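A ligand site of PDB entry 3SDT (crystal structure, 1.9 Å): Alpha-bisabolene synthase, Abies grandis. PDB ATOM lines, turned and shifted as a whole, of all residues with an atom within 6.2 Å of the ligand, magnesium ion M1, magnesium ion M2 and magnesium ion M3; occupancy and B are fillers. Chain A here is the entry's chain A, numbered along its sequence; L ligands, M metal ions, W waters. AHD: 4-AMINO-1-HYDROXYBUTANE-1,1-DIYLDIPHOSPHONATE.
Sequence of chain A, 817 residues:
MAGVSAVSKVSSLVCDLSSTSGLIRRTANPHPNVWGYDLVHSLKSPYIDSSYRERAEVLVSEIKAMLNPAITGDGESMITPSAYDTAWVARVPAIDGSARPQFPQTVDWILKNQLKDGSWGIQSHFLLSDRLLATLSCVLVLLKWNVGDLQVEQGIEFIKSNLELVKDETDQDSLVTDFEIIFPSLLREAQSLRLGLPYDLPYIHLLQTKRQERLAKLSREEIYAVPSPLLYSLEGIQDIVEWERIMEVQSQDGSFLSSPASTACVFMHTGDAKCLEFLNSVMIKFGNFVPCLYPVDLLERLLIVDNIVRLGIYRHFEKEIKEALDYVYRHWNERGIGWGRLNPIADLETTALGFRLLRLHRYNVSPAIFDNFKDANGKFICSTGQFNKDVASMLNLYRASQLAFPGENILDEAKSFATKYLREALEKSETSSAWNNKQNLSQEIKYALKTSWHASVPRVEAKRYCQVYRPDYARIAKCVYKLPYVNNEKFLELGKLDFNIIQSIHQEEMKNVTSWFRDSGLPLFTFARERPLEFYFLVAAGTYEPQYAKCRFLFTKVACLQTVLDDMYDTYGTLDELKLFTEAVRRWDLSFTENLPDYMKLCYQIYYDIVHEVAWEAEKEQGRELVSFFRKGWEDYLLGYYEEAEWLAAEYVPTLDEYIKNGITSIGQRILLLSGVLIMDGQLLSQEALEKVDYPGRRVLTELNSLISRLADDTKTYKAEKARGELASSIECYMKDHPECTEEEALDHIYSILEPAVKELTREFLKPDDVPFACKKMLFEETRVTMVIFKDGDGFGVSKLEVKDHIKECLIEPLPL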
ATOM      1  N   ARG A 531      13.978   7.440  16.524  1.00  0.00           N
ATOM      2  CA  ARG A 531      13.258   7.444  17.803  1.00  0.00           C
ATOM      3  C   ARG A 531      11.879   8.114  17.753  1.00  0.00           C
ATOM      4  O   ARG A 531      11.487   8.785  18.709  1.00  0.00           O
ATOM      5  CB  ARG A 531      14.100   8.161  18.874  1.00  0.00           C
ATOM      6  CG  ARG A 531      15.457   7.542  19.128  1.00  0.00           C
ATOM      7  CD  ARG A 531      16.030   8.067  20.434  1.00  0.00           C
ATOM      8  NE  ARG A 531      16.752   9.320  20.254  1.00  0.00           N
ATOM      9  CZ  ARG A 531      16.972  10.213  21.214  1.00  0.00           C
ATOM     10  NH1 ARG A 531      16.508   9.994  22.442  1.00  0.00           N
ATOM     11  NH2 ARG A 531      17.649  11.313  20.947  1.00  0.00           N
ATOM     12  N   GLN A 562      15.627  17.227  14.941  1.00  0.00           N
ATOM     13  CA  GLN A 562      16.665  17.697  15.849  1.00  0.00           C
ATOM     14  C   GLN A 562      17.657  16.608  16.240  1.00  0.00           C
ATOM     15  O   GLN A 562      18.845  16.872  16.377  1.00  0.00           O
ATOM     16  CB  GLN A 562      16.038  18.272  17.122  1.00  0.00           C
ATOM     17  CG  GLN A 562      15.484  19.660  16.982  1.00  0.00           C
ATOM     18  CD  GLN A 562      15.063  20.206  18.333  1.00  0.00           C
ATOM     19  OE1 GLN A 562      14.616  19.457  19.187  1.00  0.00           O
ATOM     20  NE2 GLN A 562      15.249  21.506  18.548  1.00  0.00           N
ATOM     21  N   THR A 563      17.179  15.381  16.411  1.00  0.00           N
ATOM     22  CA  THR A 563      18.106  14.318  16.801  1.00  0.00           C
ATOM     23  C   THR A 563      19.104  14.051  15.675  1.00  0.00           C
ATOM     24  O   THR A 563      20.261  13.683  15.928  1.00  0.00           O
ATOM     25  CB  THR A 563      17.378  13.028  17.230  1.00  0.00           C
ATOM     26  OG1 THR A 563      18.280  12.203  17.986  1.00  0.00           O
ATOM     27  CG2 THR A 563      16.863  12.250  16.036  1.00  0.00           C
ATOM     28  N   ASP A 566      21.492  17.199  15.775  1.00  0.00           N
ATOM     29  CA  ASP A 566      22.373  17.052  16.928  1.00  0.00           C
ATOM     30  C   ASP A 566      23.540  16.105  16.649  1.00  0.00           C
ATOM     31  O   ASP A 566      24.722  16.445  16.878  1.00  0.00           O
ATOM     32  CB  ASP A 566      21.577  16.589  18.147  1.00  0.00           C
ATOM     33  CG  ASP A 566      22.441  16.410  19.362  1.00  0.00           C
ATOM     34  OD1 ASP A 566      22.997  17.421  19.814  1.00  0.00           O
ATOM     35  OD2 ASP A 566      22.563  15.264  19.852  1.00  0.00           O
ATOM     36  N   ASP A 567      23.233  14.906  16.156  1.00  0.00           N
ATOM     37  CA  ASP A 567      24.279  13.931  15.827  1.00  0.00           C
ATOM     38  C   ASP A 567      25.216  14.466  14.744  1.00  0.00           C
ATOM     39  O   ASP A 567      26.442  14.227  14.783  1.00  0.00           O
ATOM     40  CB  ASP A 567      23.667  12.586  15.382  1.00  0.00           C
ATOM     41  CG  ASP A 567      22.890  11.887  16.504  1.00  0.00           C
ATOM     42  OD1 ASP A 567      22.935  12.337  17.666  1.00  0.00           O
ATOM     43  OD2 ASP A 567      22.238  10.851  16.212  1.00  0.00           O
ATOM     44  N   ASP A 570      27.434  17.333  16.570  1.00  0.00           N
ATOM     45  CA  ASP A 570      28.286  16.974  17.704  1.00  0.00           C
ATOM     46  C   ASP A 570      29.019  15.645  17.528  1.00  0.00           C
ATOM     47  O   ASP A 570      29.730  15.207  18.420  1.00  0.00           O
ATOM     48  CB  ASP A 570      27.512  17.004  19.038  1.00  0.00           C
ATOM     49  CG  ASP A 570      26.514  15.874  19.179  1.00  0.00           C
ATOM     50  OD1 ASP A 570      26.695  14.832  18.511  1.00  0.00           O
ATOM     51  OD2 ASP A 570      25.550  16.019  19.965  1.00  0.00           O
ATOM     52  N   THR A 571      28.868  15.014  16.362  1.00  0.00           N
ATOM     53  CA  THR A 571      29.481  13.721  16.136  1.00  0.00           C
ATOM     54  C   THR A 571      29.923  13.494  14.690  1.00  0.00           C
ATOM     55  O   THR A 571      31.120  13.414  14.408  1.00  0.00           O
ATOM     56  CB  THR A 571      28.556  12.554  16.598  1.00  0.00           C
ATOM     57  OG1 THR A 571      28.299  12.683  18.000  1.00  0.00           O
ATOM     58  CG2 THR A 571      29.197  11.203  16.323  1.00  0.00           C
ATOM     59  N   TYR A 641      24.801  25.103  18.077  1.00  0.00           N
ATOM     60  CA  TYR A 641      25.467  23.860  17.683  1.00  0.00           C
ATOM     61  C   TYR A 641      26.831  24.134  17.077  1.00  0.00           C
ATOM     62  O   TYR A 641      27.795  23.406  17.326  1.00  0.00           O
ATOM     63  CB  TYR A 641      24.634  23.104  16.649  1.00  0.00           C
ATOM     64  CG  TYR A 641      23.593  22.184  17.227  1.00  0.00           C
ATOM     65  CD1 TYR A 641      23.609  21.825  18.578  1.00  0.00           C
ATOM     66  CD2 TYR A 641      22.584  21.660  16.430  1.00  0.00           C
ATOM     67  CE1 TYR A 641      22.636  20.980  19.112  1.00  0.00           C
ATOM     68  CE2 TYR A 641      21.613  20.812  16.955  1.00  0.00           C
ATOM     69  CZ  TYR A 641      21.642  20.467  18.282  1.00  0.00           C
ATOM     70  OH  TYR A 641      20.682  19.626  18.796  1.00  0.00           O
ATOM     71  N   GLU A 644      29.513  24.952  19.534  1.00  0.00           N
ATOM     72  CA  GLU A 644      29.873  23.688  20.172  1.00  0.00           C
ATOM     73  C   GLU A 644      30.782  22.879  19.247  1.00  0.00           C
ATOM     74  O   GLU A 644      31.729  22.236  19.701  1.00  0.00           O
ATOM     75  CB  GLU A 644      28.598  22.895  20.449  1.00  0.00           C
ATOM     76  CG  GLU A 644      28.670  21.941  21.618  1.00  0.00           C
ATOM     77  CD  GLU A 644      27.324  21.305  21.933  1.00  0.00           C
ATOM     78  OE1 GLU A 644      27.037  21.052  23.115  1.00  0.00           O
ATOM     79  OE2 GLU A 644      26.537  21.072  20.976  1.00  0.00           O
ATOM     80  N   TYR A 659      29.430  27.182  29.294  1.00  0.00           N
ATOM     81  CA  TYR A 659      28.777  25.925  28.950  1.00  0.00           C
ATOM     82  C   TYR A 659      27.264  26.049  29.072  1.00  0.00           C
ATOM     83  O   TYR A 659      26.508  25.530  28.232  1.00  0.00           O
ATOM     84  CB  TYR A 659      29.280  24.821  29.878  1.00  0.00           C
ATOM     85  CG  TYR A 659      28.560  23.514  29.677  1.00  0.00           C
ATOM     86  CD1 TYR A 659      29.005  22.589  28.744  1.00  0.00           C
ATOM     87  CD2 TYR A 659      27.425  23.199  30.413  1.00  0.00           C
ATOM     88  CE1 TYR A 659      28.349  21.387  28.554  1.00  0.00           C
ATOM     89  CE2 TYR A 659      26.757  22.008  30.226  1.00  0.00           C
ATOM     90  CZ  TYR A 659      27.230  21.098  29.295  1.00  0.00           C
ATOM     91  OH  TYR A 659      26.572  19.908  29.110  1.00  0.00           O
ATOM     92  N   SER A 666      21.587  25.539  22.756  1.00  0.00           N
ATOM     93  CA  SER A 666      21.849  24.412  21.865  1.00  0.00           C
ATOM     94  C   SER A 666      21.153  23.122  22.290  1.00  0.00           C
ATOM     95  O   SER A 666      21.104  22.164  21.521  1.00  0.00           O
ATOM     96  CB  SER A 666      23.365  24.178  21.706  1.00  0.00           C
ATOM     97  OG  SER A 666      23.928  23.789  22.939  1.00  0.00           O
ATOM     98  N   ILE A 667      20.606  23.065  23.509  1.00  0.00           N
ATOM     99  CA  ILE A 667      19.936  21.850  23.958  1.00  0.00           C
ATOM    100  C   ILE A 667      18.714  21.572  23.061  1.00  0.00           C
ATOM    101  O   ILE A 667      18.301  20.424  22.905  1.00  0.00           O
ATOM    102  CB  ILE A 667      19.529  21.907  25.460  1.00  0.00           C
ATOM    103  CG1 ILE A 667      19.079  20.526  25.960  1.00  0.00           C
ATOM    104  CG2 ILE A 667      18.442  22.927  25.688  1.00  0.00           C
ATOM    105  CD1 ILE A 667      20.184  19.497  26.053  1.00  0.00           C
ATOM    106  N   GLY A 668      18.163  22.622  22.466  1.00  0.00           N
ATOM    107  CA  GLY A 668      17.152  22.462  21.435  1.00  0.00           C
ATOM    108  C   GLY A 668      15.722  22.485  21.934  1.00  0.00           C
ATOM    109  O   GLY A 668      14.774  22.468  21.137  1.00  0.00           O
ATOM    110  N   ARG A 710      19.193  20.527  30.051  1.00  0.00           N
ATOM    111  CA  ARG A 710      20.646  20.438  29.894  1.00  0.00           C
ATOM    112  C   ARG A 710      21.312  19.842  31.123  1.00  0.00           C
ATOM    113  O   ARG A 710      22.127  18.914  31.031  1.00  0.00           O
ATOM    114  CB  ARG A 710      21.236  21.819  29.597  1.00  0.00           C
ATOM    115  CG  ARG A 710      22.786  21.879  29.647  1.00  0.00           C
ATOM    116  CD  ARG A 710      23.411  21.168  28.442  1.00  0.00           C
ATOM    117  NE  ARG A 710      23.323  19.719  28.559  1.00  0.00           N
ATOM    118  CZ  ARG A 710      23.524  18.874  27.545  1.00  0.00           C
ATOM    119  NH1 ARG A 710      23.815  19.334  26.346  1.00  0.00           N
ATOM    120  NH2 ARG A 710      23.411  17.562  27.750  1.00  0.00           N
ATOM    121  N   ASP A 713      20.085  16.237  32.108  1.00  0.00           N
ATOM    122  CA  ASP A 713      20.751  15.349  31.169  1.00  0.00           C
ATOM    123  C   ASP A 713      22.173  15.061  31.668  1.00  0.00           C
ATOM    124  O   ASP A 713      22.588  13.904  31.773  1.00  0.00           O
ATOM    125  CB  ASP A 713      20.757  15.968  29.765  1.00  0.00           C
ATOM    126  CG  ASP A 713      21.513  15.122  28.744  1.00  0.00           C
ATOM    127  OD1 ASP A 713      22.652  14.701  29.033  1.00  0.00           O
ATOM    128  OD2 ASP A 713      20.977  14.887  27.638  1.00  0.00           O
ATOM    129  N   ASP A 714      22.910  16.121  31.980  1.00  0.00           N
ATOM    130  CA  ASP A 714      24.288  15.957  32.449  1.00  0.00           C
ATOM    131  C   ASP A 714      24.382  15.091  33.712  1.00  0.00           C
ATOM    132  O   ASP A 714      25.259  14.225  33.806  1.00  0.00           O
ATOM    133  CB  ASP A 714      24.926  17.334  32.715  1.00  0.00           C
ATOM    134  CG  ASP A 714      25.297  18.049  31.434  1.00  0.00           C
ATOM    135  OD1 ASP A 714      25.017  17.493  30.355  1.00  0.00           O
ATOM    136  OD2 ASP A 714      25.862  19.167  31.504  1.00  0.00           O
ATOM    137  N   THR A 717      23.815  11.471  32.759  1.00  0.00           N
ATOM    138  CA  THR A 717      24.801  10.912  31.830  1.00  0.00           C
ATOM    139  C   THR A 717      26.201  11.412  32.212  1.00  0.00           C
ATOM    140  O   THR A 717      26.632  11.209  33.341  1.00  0.00           O
ATOM    141  CB  THR A 717      24.431  11.231  30.361  1.00  0.00           C
ATOM    142  OG1 THR A 717      24.205  12.638  30.200  1.00  0.00           O
ATOM    143  CG2 THR A 717      23.140  10.514  30.003  1.00  0.00           C
ATOM    144  N   LEU A 727      33.114  16.276  23.886  1.00  0.00           N
ATOM    145  CA  LEU A 727      32.523  17.448  24.505  1.00  0.00           C
ATOM    146  C   LEU A 727      32.344  17.269  26.010  1.00  0.00           C
ATOM    147  O   LEU A 727      31.700  16.309  26.451  1.00  0.00           O
ATOM    148  CB  LEU A 727      31.189  17.798  23.863  1.00  0.00           C
ATOM    149  CG  LEU A 727      31.266  18.505  22.509  1.00  0.00           C
ATOM    150  CD1 LEU A 727      29.885  18.573  21.836  1.00  0.00           C
ATOM    151  CD2 LEU A 727      31.881  19.892  22.659  1.00  0.00           C
ATOM    152  N   PHE A 790      15.398  11.611  32.915  1.00  0.00           N
ATOM    153  CA  PHE A 790      16.693  11.864  33.522  1.00  0.00           C
ATOM    154  C   PHE A 790      16.743  11.768  35.059  1.00  0.00           C
ATOM    155  O   PHE A 790      17.699  12.230  35.671  1.00  0.00           O
ATOM    156  CB  PHE A 790      17.203  13.243  33.090  1.00  0.00           C
ATOM    157  CG  PHE A 790      17.417  13.361  31.614  1.00  0.00           C
ATOM    158  CD1 PHE A 790      18.106  12.382  30.917  1.00  0.00           C
ATOM    159  CD2 PHE A 790      16.908  14.443  30.920  1.00  0.00           C
ATOM    160  CE1 PHE A 790      18.303  12.486  29.551  1.00  0.00           C
ATOM    161  CE2 PHE A 790      17.106  14.553  29.541  1.00  0.00           C
ATOM    162  CZ  PHE A 790      17.802  13.572  28.867  1.00  0.00           C
HETATM  163  C2  AHD L   1      21.007  15.947  22.766  1.00  0.00           C
HETATM  164  C3  AHD L   1      19.532  15.918  22.430  1.00  0.00           C
HETATM  165  C7  AHD L   1      21.208  15.395  24.159  1.00  0.00           C
HETATM  166  C8  AHD L   1      22.616  14.845  24.357  1.00  0.00           C
HETATM  167  O12 AHD L   1      24.063  12.548  24.177  1.00  0.00           O
HETATM  168  P9  AHD L   1      22.785  13.197  23.551  1.00  0.00           P
HETATM  169  O10 AHD L   1      23.040  13.374  22.021  1.00  0.00           O
HETATM  170  O11 AHD L   1      21.625  12.300  23.781  1.00  0.00           O
HETATM  171  P14 AHD L   1      23.936  16.003  23.812  1.00  0.00           P
HETATM  172  O15 AHD L   1      24.117  16.030  22.242  1.00  0.00           O
HETATM  173  O16 AHD L   1      25.220  15.425  24.458  1.00  0.00           O
HETATM  174  O17 AHD L   1      23.697  17.394  24.281  1.00  0.00           O
HETATM  175  O13 AHD L   1      22.820  14.676  25.715  1.00  0.00           O
HETATM  176  N4  AHD L   1      18.925  17.192  22.750  1.00  0.00           N
HETATM  177 MG    MG M   1      24.259  14.509  20.942  1.00  0.00          MG
HETATM  178 MG    MG M   2      24.789  13.710  25.674  1.00  0.00          MG
HETATM  179 MG    MG M   3      24.646  17.602  20.989  1.00  0.00          MG
HETATM  180  O   HOH W   1      24.695  13.174  19.502  1.00  0.00           O
HETATM  181  O   HOH W   2      27.386  16.877  24.353  1.00  0.00           O
HETATM  182  O   HOH W   3      15.765  18.696  22.776  1.00  0.00           O
HETATM  183  O   HOH W   4      24.180  12.212  26.969  1.00  0.00           O
HETATM  184  O   HOH W   5      26.684  12.981  25.447  1.00  0.00           O
HETATM  185  O   HOH W   6      21.821  11.041  20.499  1.00  0.00           O
HETATM  186  O   HOH W   7      23.421  18.779  22.203  1.00  0.00           O
HETATM  187  O   HOH W   8      25.005  19.258  19.832  1.00  0.00           O
HETATM  188  O   HOH W   9      20.618  12.110  26.492  1.00  0.00           O
HETATM  189  O   HOH W  10      25.203  14.967  27.295  1.00  0.00           O
HETATM  190  O   HOH W  11      19.214  12.384  22.768  1.00  0.00           O
HETATM  191  O   HOH W  12      25.951  14.056  22.099  1.00  0.00           O
HETATM  192  O   HOH W  13      20.762  19.254  21.291  1.00  0.00           O
HETATM  193  O   HOH W  14      18.729  15.810  26.400  1.00  0.00           O
HETATM  194  O   HOH W  15      26.296  18.060  22.166  1.00  0.00           O
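Merely in contact with magnesium ion M3: Glu 644 (3.95 Å).
Two residues have an atom within 4 Å of magnesium ion M1: Asp 566 and Asp 570.
OD1 of Asp 566 lies close to OH of Tyr 641 (3.4 Å). OD1 of Asp 570 sits at hydrogen-bond distance from OG1 of Thr 571 (2.7 Å). OD1 of Asp 713 lies within salt-bridge range of NH2 of Arg 710 (3.2 Å). The backbone carbonyl oxygen (O) of Asp 713 sits at hydrogen-bond distance from the side-chain hydroxyl (OG1) of Thr 717, at 2.6 Å. NH2 of Arg 710 is in salt-bridge range of OD1 of Asp 714 (3.1 Å). NE of Arg 710 sits at hydrogen-bond distance from OH of Tyr 659, 3.3 Å away.
Magnesium ion M1 is bound by O10 of the ligand (2.0 Å), O15 of the ligand (2.0 Å), water W1 (2.0 Å), water W12 (2.1 Å), OD2 of Asp 566 (2.2 Å) and OD2 of Asp 570 (2.2 Å). Magnesium ion M1 has six donor atoms within binding distance.
Water W1 bridges OD1 of Asp 567 and OD1 of Asp 570. Water W10 bridges OD1 of Asp 713 (3.1 Å) and NH2 of Arg 710 (3.2 Å). Water W15 bridges the side-chain carboxylate (OE1) of Glu 644 and an oxygen (O17) of the ligand. Water W11 bridges O11 of the ligand (2.6 Å) and NH2 of Arg 531 (2.6 Å). Water W9 lies within hydrogen-bond range of an oxygen (O11) of the ligand (2.9 Å) and the side-chain carboxylate of Asp 713 (3.0 Å). Water W3 bridges O of Ile 667 and N4 of the ligand.
Magnesium ion M2 is bound by O12 of the ligand, water W5, water W4, water W10, O16 of the ligand and O13 of the ligand. Magnesium ion M2 has six donor atoms within binding distance.
Magnesium ion M3 is bound by OD1 of Asp 566 (2.0 Å). Magnesium ion M3 is bound by water W8 (2.1 Å). Water W15 is bound to magnesium ion M3 (2.1 Å). Magnesium ion M3 is bound by O15 of the ligand, 2.1 Å away. Water W7 is bound to magnesium ion M3. The side-chain carboxylate (OD2) of Asp 570 is bound to magnesium ion M3, at 2.1 Å.
No residue comes within 4 Å of magnesium ion M2. The nearest printed residue that does not touch magnesium ion M2 is Asp 713 (4.1 Å).
The side-chain carboxylate (OD2) of Asp 713 sits close to an oxygen (O13) of the ligand (2.7 Å). The guanidinium group of Arg 710 is in salt-bridge range of an oxygen (O17) of the ligand, at 2.8 Å. The backbone carbonyl oxygen of Ile 667 lies within hydrogen-bond range of a nitrogen (N4) of the ligand, at 3.3 Å.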
